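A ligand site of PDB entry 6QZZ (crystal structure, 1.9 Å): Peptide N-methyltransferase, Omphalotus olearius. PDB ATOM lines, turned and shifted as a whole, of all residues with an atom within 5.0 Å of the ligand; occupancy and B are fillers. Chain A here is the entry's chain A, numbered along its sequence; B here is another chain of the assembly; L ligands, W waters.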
ATOM      1  N   ILE A  18      -6.091 -14.718 -23.041  1.00  0.00           N
ATOM      2  CA  ILE A  18      -6.254 -15.994 -23.783  1.00  0.00           C
ATOM      3  C   ILE A  18      -6.196 -15.708 -25.284  1.00  0.00           C
ATOM      4  O   ILE A  18      -5.448 -16.409 -25.981  1.00  0.00           O
ATOM      5  CB  ILE A  18      -7.553 -16.704 -23.367  1.00  0.00           C
ATOM      6  CG1 ILE A  18      -7.515 -17.106 -21.888  1.00  0.00           C
ATOM      7  CG2 ILE A  18      -7.811 -17.891 -24.264  1.00  0.00           C
ATOM      8  CD1 ILE A  18      -6.421 -18.074 -21.494  1.00  0.00           C
ATOM      9  N   ILE A  43       0.775 -19.522 -25.868  1.00  0.00           N
ATOM     10  CA  ILE A  43       0.238 -20.608 -26.744  1.00  0.00           C
ATOM     11  C   ILE A  43       0.584 -20.285 -28.191  1.00  0.00           C
ATOM     12  O   ILE A  43       1.165 -21.172 -28.884  1.00  0.00           O
ATOM     13  CB  ILE A  43      -1.287 -20.784 -26.573  1.00  0.00           C
ATOM     14  CG1 ILE A  43      -1.589 -21.548 -25.279  1.00  0.00           C
ATOM     15  CG2 ILE A  43      -1.903 -21.475 -27.771  1.00  0.00           C
ATOM     16  CD1 ILE A  43      -2.948 -22.218 -25.279  1.00  0.00           C
ATOM     17  N   TYR A  97       0.512 -17.263 -20.298  1.00  0.00           N
ATOM     18  CA  TYR A  97      -0.798 -17.292 -21.001  1.00  0.00           C
ATOM     19  C   TYR A  97      -1.891 -17.051 -19.954  1.00  0.00           C
ATOM     20  O   TYR A  97      -1.783 -17.599 -18.833  1.00  0.00           O
ATOM     21  CB  TYR A  97      -0.881 -18.687 -21.615  1.00  0.00           C
ATOM     22  CG  TYR A  97      -2.176 -19.128 -22.228  1.00  0.00           C
ATOM     23  CD1 TYR A  97      -2.576 -18.613 -23.452  1.00  0.00           C
ATOM     24  CD2 TYR A  97      -2.888 -20.180 -21.687  1.00  0.00           C
ATOM     25  CE1 TYR A  97      -3.726 -19.080 -24.086  1.00  0.00           C
ATOM     26  CE2 TYR A  97      -4.030 -20.656 -22.308  1.00  0.00           C
ATOM     27  CZ  TYR A  97      -4.459 -20.101 -23.510  1.00  0.00           C
ATOM     28  OH  TYR A  97      -5.588 -20.557 -24.149  1.00  0.00           O
ATOM     29  N   GLY A  98      -2.926 -16.287 -20.314  1.00  0.00           N
ATOM     30  CA  GLY A  98      -4.098 -16.039 -19.465  1.00  0.00           C
ATOM     31  C   GLY A  98      -3.768 -15.114 -18.322  1.00  0.00           C
ATOM     32  O   GLY A  98      -3.124 -14.078 -18.549  1.00  0.00           O
ATOM     33  N   HIS A  99      -4.218 -15.482 -17.133  1.00  0.00           N
ATOM     34  CA  HIS A  99      -3.784 -14.904 -15.846  1.00  0.00           C
ATOM     35  C   HIS A  99      -2.579 -15.720 -15.369  1.00  0.00           C
ATOM     36  O   HIS A  99      -2.640 -16.951 -15.305  1.00  0.00           O
ATOM     37  CB  HIS A  99      -4.963 -14.940 -14.884  1.00  0.00           C
ATOM     38  CG  HIS A  99      -4.751 -14.323 -13.552  1.00  0.00           C
ATOM     39  ND1 HIS A  99      -3.679 -14.650 -12.753  1.00  0.00           N
ATOM     40  CD2 HIS A  99      -5.549 -13.500 -12.825  1.00  0.00           C
ATOM     41  CE1 HIS A  99      -3.777 -14.009 -11.607  1.00  0.00           C
ATOM     42  NE2 HIS A  99      -4.930 -13.300 -11.616  1.00  0.00           N
ATOM     43  N   PRO A 100      -1.439 -15.075 -15.062  1.00  0.00           N
ATOM     44  CA  PRO A 100      -0.197 -15.816 -14.822  1.00  0.00           C
ATOM     45  C   PRO A 100      -0.178 -16.578 -13.488  1.00  0.00           C
ATOM     46  O   PRO A 100       0.788 -17.292 -13.240  1.00  0.00           O
ATOM     47  CB  PRO A 100       0.852 -14.710 -14.839  1.00  0.00           C
ATOM     48  CG  PRO A 100       0.116 -13.511 -14.267  1.00  0.00           C
ATOM     49  CD  PRO A 100      -1.260 -13.615 -14.919  1.00  0.00           C
ATOM     50  N   VAL A 102      -3.205 -18.251 -12.338  1.00  0.00           N
ATOM     51  CA  VAL A 102      -4.390 -19.147 -12.374  1.00  0.00           C
ATOM     52  C   VAL A 102      -3.947 -20.446 -13.040  1.00  0.00           C
ATOM     53  O   VAL A 102      -3.631 -20.429 -14.248  1.00  0.00           O
ATOM     54  CB  VAL A 102      -5.566 -18.456 -13.083  1.00  0.00           C
ATOM     55  CG1 VAL A 102      -6.697 -19.403 -13.417  1.00  0.00           C
ATOM     56  CG2 VAL A 102      -6.077 -17.283 -12.274  1.00  0.00           C
ATOM     57  N   PHE A 103      -3.843 -21.522 -12.253  1.00  0.00           N
ATOM     58  CA  PHE A 103      -3.350 -22.838 -12.686  1.00  0.00           C
ATOM     59  C   PHE A 103      -1.925 -22.658 -13.257  1.00  0.00           C
ATOM     60  O   PHE A 103      -1.682 -23.131 -14.360  1.00  0.00           O
ATOM     61  CB  PHE A 103      -4.394 -23.461 -13.644  1.00  0.00           C
ATOM     62  CG  PHE A 103      -5.749 -23.667 -12.999  1.00  0.00           C
ATOM     63  CD1 PHE A 103      -6.643 -22.622 -12.863  1.00  0.00           C
ATOM     64  CD2 PHE A 103      -6.134 -24.913 -12.511  1.00  0.00           C
ATOM     65  CE1 PHE A 103      -7.892 -22.800 -12.257  1.00  0.00           C
ATOM     66  CE2 PHE A 103      -7.369 -25.093 -11.898  1.00  0.00           C
ATOM     67  CZ  PHE A 103      -8.242 -24.040 -11.754  1.00  0.00           C
ATOM     68  N   VAL A 104      -1.048 -21.933 -12.559  1.00  0.00           N
ATOM     69  CA  VAL A 104       0.371 -21.725 -12.989  1.00  0.00           C
ATOM     70  C   VAL A 104       1.273 -21.989 -11.782  1.00  0.00           C
ATOM     71  O   VAL A 104       1.222 -21.227 -10.801  1.00  0.00           O
ATOM     72  CB  VAL A 104       0.650 -20.316 -13.576  1.00  0.00           C
ATOM     73  CG1 VAL A 104       2.089 -20.195 -14.086  1.00  0.00           C
ATOM     74  CG2 VAL A 104      -0.339 -19.940 -14.675  1.00  0.00           C
ATOM     75  N   VAL A 127      -6.431 -11.739 -17.900  1.00  0.00           N
ATOM     76  CA  VAL A 127      -7.708 -12.391 -18.300  1.00  0.00           C
ATOM     77  C   VAL A 127      -7.496 -13.899 -18.355  1.00  0.00           C
ATOM     78  O   VAL A 127      -6.676 -14.361 -19.167  1.00  0.00           O
ATOM     79  CB  VAL A 127      -8.168 -11.813 -19.649  1.00  0.00           C
ATOM     80  CG1 VAL A 127      -9.363 -12.575 -20.192  1.00  0.00           C
ATOM     81  CG2 VAL A 127      -8.455 -10.323 -19.553  1.00  0.00           C
ATOM     82  N   SER A 128      -8.218 -14.655 -17.529  1.00  0.00           N
ATOM     83  CA  SER A 128      -8.139 -16.128 -17.462  1.00  0.00           C
ATOM     84  C   SER A 128      -9.110 -16.749 -18.463  1.00  0.00           C
ATOM     85  O   SER A 128     -10.013 -16.036 -18.963  1.00  0.00           O
ATOM     86  CB  SER A 128      -8.475 -16.615 -16.088  1.00  0.00           C
ATOM     87  OG  SER A 128      -9.856 -16.438 -15.854  1.00  0.00           O
ATOM     88  N   ALA A 129      -8.979 -18.060 -18.661  1.00  0.00           N
ATOM     89  CA  ALA A 129      -9.914 -18.868 -19.460  1.00  0.00           C
ATOM     90  C   ALA A 129     -11.302 -18.794 -18.814  1.00  0.00           C
ATOM     91  O   ALA A 129     -12.308 -18.860 -19.548  1.00  0.00           O
ATOM     92  CB  ALA A 129      -9.426 -20.283 -19.573  1.00  0.00           C
ATOM     93  N   GLU A 130     -11.366 -18.670 -17.496  1.00  0.00           N
ATOM     94  CA  GLU A 130     -12.659 -18.576 -16.775  1.00  0.00           C
ATOM     95  C   GLU A 130     -13.308 -17.200 -17.056  1.00  0.00           C
ATOM     96  O   GLU A 130     -14.524 -17.154 -17.308  1.00  0.00           O
ATOM     97  CB  GLU A 130     -12.465 -18.823 -15.277  1.00  0.00           C
ATOM     98  CG  GLU A 130     -13.780 -18.746 -14.523  1.00  0.00           C
ATOM     99  CD  GLU A 130     -13.718 -19.294 -13.121  1.00  0.00           C
ATOM    100  OE1 GLU A 130     -13.204 -18.604 -12.232  1.00  0.00           O
ATOM    101  OE2 GLU A 130     -14.221 -20.390 -12.921  1.00  0.00           O
ATOM    102  N   LEU A 169     -14.598 -26.678 -14.627  1.00  0.00           N
ATOM    103  CA  LEU A 169     -13.468 -27.655 -14.530  1.00  0.00           C
ATOM    104  C   LEU A 169     -12.376 -27.344 -15.570  1.00  0.00           C
ATOM    105  O   LEU A 169     -12.664 -27.396 -16.770  1.00  0.00           O
ATOM    106  CB  LEU A 169     -14.041 -29.062 -14.723  1.00  0.00           C
ATOM    107  CG  LEU A 169     -15.074 -29.506 -13.686  1.00  0.00           C
ATOM    108  CD1 LEU A 169     -15.496 -30.938 -13.943  1.00  0.00           C
ATOM    109  CD2 LEU A 169     -14.523 -29.349 -12.276  1.00  0.00           C
ATOM    110  N   PHE A 170     -11.165 -27.040 -15.103  1.00  0.00           N
ATOM    111  CA  PHE A 170      -9.927 -26.820 -15.903  1.00  0.00           C
ATOM    112  C   PHE A 170      -9.131 -28.128 -16.035  1.00  0.00           C
ATOM    113  O   PHE A 170      -9.279 -28.987 -15.162  1.00  0.00           O
ATOM    114  CB  PHE A 170      -8.997 -25.846 -15.174  1.00  0.00           C
ATOM    115  CG  PHE A 170      -9.275 -24.374 -15.340  1.00  0.00           C
ATOM    116  CD1 PHE A 170     -10.425 -23.801 -14.799  1.00  0.00           C
ATOM    117  CD2 PHE A 170      -8.353 -23.544 -15.953  1.00  0.00           C
ATOM    118  CE1 PHE A 170     -10.663 -22.444 -14.930  1.00  0.00           C
ATOM    119  CE2 PHE A 170      -8.595 -22.192 -16.092  1.00  0.00           C
ATOM    120  CZ  PHE A 170      -9.747 -21.633 -15.568  1.00  0.00           C
ATOM    121  N   GLN A 171      -8.270 -28.214 -17.052  1.00  0.00           N
ATOM    122  CA  GLN A 171      -7.298 -29.339 -17.268  1.00  0.00           C
ATOM    123  C   GLN A 171      -8.074 -30.646 -17.369  1.00  0.00           C
ATOM    124  O   GLN A 171      -7.573 -31.674 -16.865  1.00  0.00           O
ATOM    125  CB  GLN A 171      -6.190 -29.341 -16.202  1.00  0.00           C
ATOM    126  CG  GLN A 171      -5.465 -28.001 -16.101  1.00  0.00           C
ATOM    127  CD  GLN A 171      -4.002 -28.008 -15.723  1.00  0.00           C
ATOM    128  OE1 GLN A 171      -3.228 -27.142 -16.140  1.00  0.00           O
ATOM    129  NE2 GLN A 171      -3.592 -28.959 -14.887  1.00  0.00           N
ATOM    130  N   VAL A 172      -9.244 -30.621 -18.042  1.00  0.00           N
ATOM    131  CA  VAL A 172     -10.082 -31.843 -18.228  1.00  0.00           C
ATOM    132  C   VAL A 172      -9.438 -32.760 -19.272  1.00  0.00           C
ATOM    133  O   VAL A 172      -9.838 -33.935 -19.331  1.00  0.00           O
ATOM    134  CB  VAL A 172     -11.529 -31.525 -18.636  1.00  0.00           C
ATOM    135  CG1 VAL A 172     -12.332 -30.883 -17.496  1.00  0.00           C
ATOM    136  CG2 VAL A 172     -11.618 -30.689 -19.891  1.00  0.00           C
ATOM    137  N   TYR A 210     -16.171 -25.925 -23.559  1.00  0.00           N
ATOM    138  CA  TYR A 210     -15.814 -24.517 -23.823  1.00  0.00           C
ATOM    139  C   TYR A 210     -14.370 -24.444 -24.299  1.00  0.00           C
ATOM    140  O   TYR A 210     -13.458 -24.903 -23.580  1.00  0.00           O
ATOM    141  CB  TYR A 210     -16.042 -23.638 -22.596  1.00  0.00           C
ATOM    142  CG  TYR A 210     -15.598 -22.224 -22.838  1.00  0.00           C
ATOM    143  CD1 TYR A 210     -16.190 -21.463 -23.836  1.00  0.00           C
ATOM    144  CD2 TYR A 210     -14.533 -21.668 -22.137  1.00  0.00           C
ATOM    145  CE1 TYR A 210     -15.760 -20.172 -24.108  1.00  0.00           C
ATOM    146  CE2 TYR A 210     -14.108 -20.385 -22.389  1.00  0.00           C
ATOM    147  CZ  TYR A 210     -14.724 -19.626 -23.372  1.00  0.00           C
ATOM    148  OH  TYR A 210     -14.285 -18.370 -23.643  1.00  0.00           O
ATOM    149  N   ILE A 211     -14.164 -23.853 -25.473  1.00  0.00           N
ATOM    150  CA  ILE A 211     -12.818 -23.410 -25.931  1.00  0.00           C
ATOM    151  C   ILE A 211     -12.930 -21.961 -26.398  1.00  0.00           C
ATOM    152  O   ILE A 211     -13.586 -21.704 -27.416  1.00  0.00           O
ATOM    153  CB  ILE A 211     -12.239 -24.298 -27.041  1.00  0.00           C
ATOM    154  CG1 ILE A 211     -12.227 -25.787 -26.659  1.00  0.00           C
ATOM    155  CG2 ILE A 211     -10.851 -23.821 -27.414  1.00  0.00           C
ATOM    156  CD1 ILE A 211     -11.905 -26.691 -27.827  1.00  0.00           C
ATOM    157  N   ALA A 212     -12.287 -21.054 -25.657  1.00  0.00           N
ATOM    158  CA  ALA A 212     -12.093 -19.646 -26.042  1.00  0.00           C
ATOM    159  C   ALA A 212     -11.304 -19.620 -27.354  1.00  0.00           C
ATOM    160  O   ALA A 212     -10.291 -20.351 -27.455  1.00  0.00           O
ATOM    161  CB  ALA A 212     -11.356 -18.895 -24.971  1.00  0.00           C
ATOM    162  N   MET A 214      -8.581 -18.473 -29.653  1.00  0.00           N
ATOM    163  CA  MET A 214      -7.200 -18.044 -29.338  1.00  0.00           C
ATOM    164  C   MET A 214      -6.706 -17.047 -30.383  1.00  0.00           C
ATOM    165  O   MET A 214      -5.736 -16.320 -30.095  1.00  0.00           O
ATOM    166  CB  MET A 214      -6.306 -19.281 -29.221  1.00  0.00           C
ATOM    167  CG  MET A 214      -6.271 -19.758 -27.777  1.00  0.00           C
ATOM    168  SD  MET A 214      -6.057 -21.490 -27.579  1.00  0.00           S
ATOM    169  CE  MET A 214      -7.332 -22.095 -28.689  1.00  0.00           C
ATOM    170  N   GLY A 241      -6.150 -30.192 -24.589  1.00  0.00           N
ATOM    171  CA  GLY A 241      -5.361 -29.423 -23.608  1.00  0.00           C
ATOM    172  C   GLY A 241      -5.935 -28.052 -23.308  1.00  0.00           C
ATOM    173  O   GLY A 241      -5.618 -27.546 -22.220  1.00  0.00           O
ATOM    174  N   VAL A 242      -6.705 -27.445 -24.224  1.00  0.00           N
ATOM    175  CA  VAL A 242      -7.281 -26.077 -24.011  1.00  0.00           C
ATOM    176  C   VAL A 242      -8.792 -26.162 -23.731  1.00  0.00           C
ATOM    177  O   VAL A 242      -9.475 -25.118 -23.820  1.00  0.00           O
ATOM    178  CB  VAL A 242      -6.981 -25.118 -25.177  1.00  0.00           C
ATOM    179  CG1 VAL A 242      -5.513 -24.765 -25.228  1.00  0.00           C
ATOM    180  CG2 VAL A 242      -7.475 -25.663 -26.522  1.00  0.00           C
ATOM    181  N   SER A 243      -9.303 -27.353 -23.425  1.00  0.00           N
ATOM    182  CA  SER A 243     -10.745 -27.588 -23.158  1.00  0.00           C
ATOM    183  C   SER A 243     -11.053 -27.282 -21.690  1.00  0.00           C
ATOM    184  O   SER A 243     -10.271 -27.679 -20.800  1.00  0.00           O
ATOM    185  CB  SER A 243     -11.158 -28.986 -23.539  1.00  0.00           C
ATOM    186  OG  SER A 243     -11.027 -29.172 -24.940  1.00  0.00           O
ATOM    187  N   THR A 244     -12.137 -26.552 -21.459  1.00  0.00           N
ATOM    188  CA  THR A 244     -12.716 -26.313 -20.115  1.00  0.00           C
ATOM    189  C   THR A 244     -14.151 -26.799 -20.153  1.00  0.00           C
ATOM    190  O   THR A 244     -14.795 -26.678 -21.209  1.00  0.00           O
ATOM    191  CB  THR A 244     -12.579 -24.843 -19.711  1.00  0.00           C
ATOM    192  OG1 THR A 244     -11.177 -24.550 -19.629  1.00  0.00           O
ATOM    193  CG2 THR A 244     -13.239 -24.540 -18.391  1.00  0.00           C
ATOM    194  N   ILE B 401      -0.172 -26.435 -23.620  1.00  0.00           N
ATOM    195  CA  ILE B 401       0.466 -25.488 -22.707  1.00  0.00           C
ATOM    196  C   ILE B 401       0.034 -25.709 -21.261  1.00  0.00           C
ATOM    197  O   ILE B 401      -0.716 -24.887 -20.715  1.00  0.00           O
ATOM    198  CB  ILE B 401       0.222 -24.021 -23.119  1.00  0.00           C
ATOM    199  CG1 ILE B 401       1.139 -23.074 -22.330  1.00  0.00           C
ATOM    200  CG2 ILE B 401      -1.253 -23.654 -22.979  1.00  0.00           C
ATOM    201  CD1 ILE B 401       1.768 -21.987 -23.159  1.00  0.00           C
ATOM    202  C7  EME B 403      -0.780 -24.931 -17.078  1.00  0.00           C
ATOM    203  N   EME B 403       0.565 -25.434 -17.414  1.00  0.00           N
ATOM    204  CA  EME B 403       1.531 -24.780 -16.529  1.00  0.00           C
ATOM    205  C   EME B 403       1.237 -25.122 -15.064  1.00  0.00           C
ATOM    206  O   EME B 403       1.772 -24.492 -14.142  1.00  0.00           O
ATOM    207  CB  EME B 403       1.611 -23.244 -16.658  1.00  0.00           C
ATOM    208  CG  EME B 403       1.212 -22.667 -18.030  1.00  0.00           C
ATOM    209  CD  EME B 403       2.405 -22.058 -18.750  1.00  0.00           C
ATOM    210  OE2 EME B 403       2.208 -21.042 -19.490  1.00  0.00           O
ATOM    211  OE1 EME B 403       3.557 -22.555 -18.609  1.00  0.00           O
HETATM  212  N1  LIG L   1      -3.112 -19.311 -16.652  1.00  0.00           N
HETATM  213  C1  LIG L   1      -4.161 -19.849 -17.587  1.00  0.00           C
HETATM  214  C2  LIG L   1      -4.490 -21.324 -17.292  1.00  0.00           C
HETATM  215  C3  LIG L   1      -3.366 -22.347 -17.484  1.00  0.00           C
HETATM  216  S1  LIG L   1      -3.885 -24.057 -17.007  1.00  0.00           S
HETATM  217  C4  LIG L   1      -5.453 -19.046 -17.398  1.00  0.00           C
HETATM  218  O1  LIG L   1      -6.560 -19.512 -17.766  1.00  0.00           O
HETATM  219  O2  LIG L   1      -5.436 -17.960 -16.840  1.00  0.00           O
HETATM  220  C5  LIG L   1      -4.541 -24.769 -18.590  1.00  0.00           C
HETATM  221  C6  LIG L   1      -6.053 -24.924 -18.602  1.00  0.00           C
HETATM  222  O3  LIG L   1      -6.699 -23.635 -18.827  1.00  0.00           O
HETATM  223  C7  LIG L   1      -6.607 -25.794 -19.719  1.00  0.00           C
HETATM  224  O4  LIG L   1      -6.495 -27.178 -19.412  1.00  0.00           O
HETATM  225  C8  LIG L   1      -8.057 -25.315 -19.752  1.00  0.00           C
HETATM  226  O5  LIG L   1      -8.836 -25.864 -18.708  1.00  0.00           O
HETATM  227  C9  LIG L   1      -7.879 -23.810 -19.594  1.00  0.00           C
HETATM  228  N2  LIG L   1      -7.751 -23.131 -20.895  1.00  0.00           N
HETATM  229  C10 LIG L   1      -6.606 -22.737 -21.539  1.00  0.00           C
HETATM  230  N3  LIG L   1      -6.823 -22.199 -22.718  1.00  0.00           N
HETATM  231  C11 LIG L   1      -8.204 -22.261 -22.880  1.00  0.00           C
HETATM  232  C12 LIG L   1      -9.059 -21.858 -23.933  1.00  0.00           C
HETATM  233  N4  LIG L   1      -8.623 -21.311 -25.067  1.00  0.00           N
HETATM  234  N5  LIG L   1     -10.387 -22.077 -23.779  1.00  0.00           N
HETATM  235  C13 LIG L   1     -10.808 -22.639 -22.634  1.00  0.00           C
HETATM  236  N6  LIG L   1     -10.098 -23.058 -21.590  1.00  0.00           N
HETATM  237  C14 LIG L   1      -8.779 -22.845 -21.773  1.00  0.00           C
HETATM  238  O   HOH W   1      -8.112 -29.281 -20.678  1.00  0.00           O
HETATM  239  O   HOH W   2      -0.718 -19.835 -18.060  1.00  0.00           O
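O of Phe 103 lies close to S1 of the ligand (3.6 Å). N6 of the ligand sits close to O of Val 242, at 3.1 Å. Residues that only touch the ligand: Ile 18, Gly 98, Val 104, Ser 128, Phe 170, Tyr 210, Ile 211 and EME 403 of chain B. Hydrophobic or aromatic side chains that line the ligand: Ile 18, Tyr 97, His 99, Val 102, Phe 103, Val 104, Ala 129, Phe 170, Tyr 210, Ala 212, Met 214 and Val 242. 20 residues have an atom within 4 Å of the ligand: Ile 18, Tyr 97, Gly 98, His 99, Val 102, Phe 103, Val 104, Ser 128, Ala 129, Phe 170, Gln 171, Tyr 210, Ile 211, Ala 212, Met 214, Gly 241, Val 242, Ser 243, Thr 244 and EME 403 of chain B. The nearest printed residue that does not touch the ligand is Ile 401 of chain B (4.4 Å).
A nitrogen (N6) of the ligand lies within hydrogen-bond range of the side-chain hydroxyl (OG1) of Thr 244 (2.7 Å). N of Gln 171 is in hydrogen-bond range of O5 of the ligand (2.9 Å). The backbone carbonyl oxygen (O) of Gly 241 sits at hydrogen-bond distance from an oxygen (O4) of the ligand (3.0 Å). N4 of the ligand sits at hydrogen-bond distance from SD of Met 214 (3.6 Å). The backbone carbonyl oxygen of Ser 243 lies within hydrogen-bond range of an oxygen (O5) of the ligand, at 3.1 Å. The backbone carbonyl oxygen (O) of His 99 lies within hydrogen-bond range of a nitrogen (N1) of the ligand (2.8 Å). An oxygen (O2) of the ligand sits at hydrogen-bond distance from the backbone NH (N) of His 99 (2.8 Å). The side-chain hydroxyl (OH) of Tyr 97 sits at hydrogen-bond distance from a nitrogen (N3) of the ligand, 2.5 Å away. The backbone carbonyl oxygen of Val 102 is in hydrogen-bond range of a nitrogen (N1) of the ligand, 2.7 Å away. An oxygen (O1) of the ligand sits at hydrogen-bond distance from the backbone NH of Ala 129, 3.0 Å away. The backbone carbonyl oxygen (O) of Tyr 97 lies within hydrogen-bond range of a nitrogen (N1) of the ligand, at 3.1 Å. A nitrogen (N5) of the ligand sits at hydrogen-bond distance from the backbone NH (N) of Ala 212 (2.9 Å). The backbone carbonyl oxygen of Ala 212 is in hydrogen-bond range of a nitrogen (N4) of the ligand, 3.1 Å away. OE1 of Gln 171 sits close to S1 of the ligand (3.3 Å).
The side-chain hydroxyl (OH) of Tyr 97 sits at hydrogen-bond distance from the side-chain sulfur (SD) of Met 214 (3.6 Å). O of Thr 244 sits at hydrogen-bond distance from N of Tyr 210. The backbone carbonyl oxygen (O) of Val 127 is in hydrogen-bond range of the backbone NH (N) of His 99. OG of Ser 128 sits close to N of Glu 130, 3.2 Å away.
Water W2 lies within hydrogen-bond range of the backbone carbonyl oxygen (O) of Tyr 97 (2.6 Å), a nitrogen (N1) of the ligand (2.8 Å) and OE2 of EME 403 of chain B (3.5 Å). Water W1 lies within hydrogen-bond range of O of Ser 243, O4 of the ligand, N of Val 172 and O of Gly 241.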
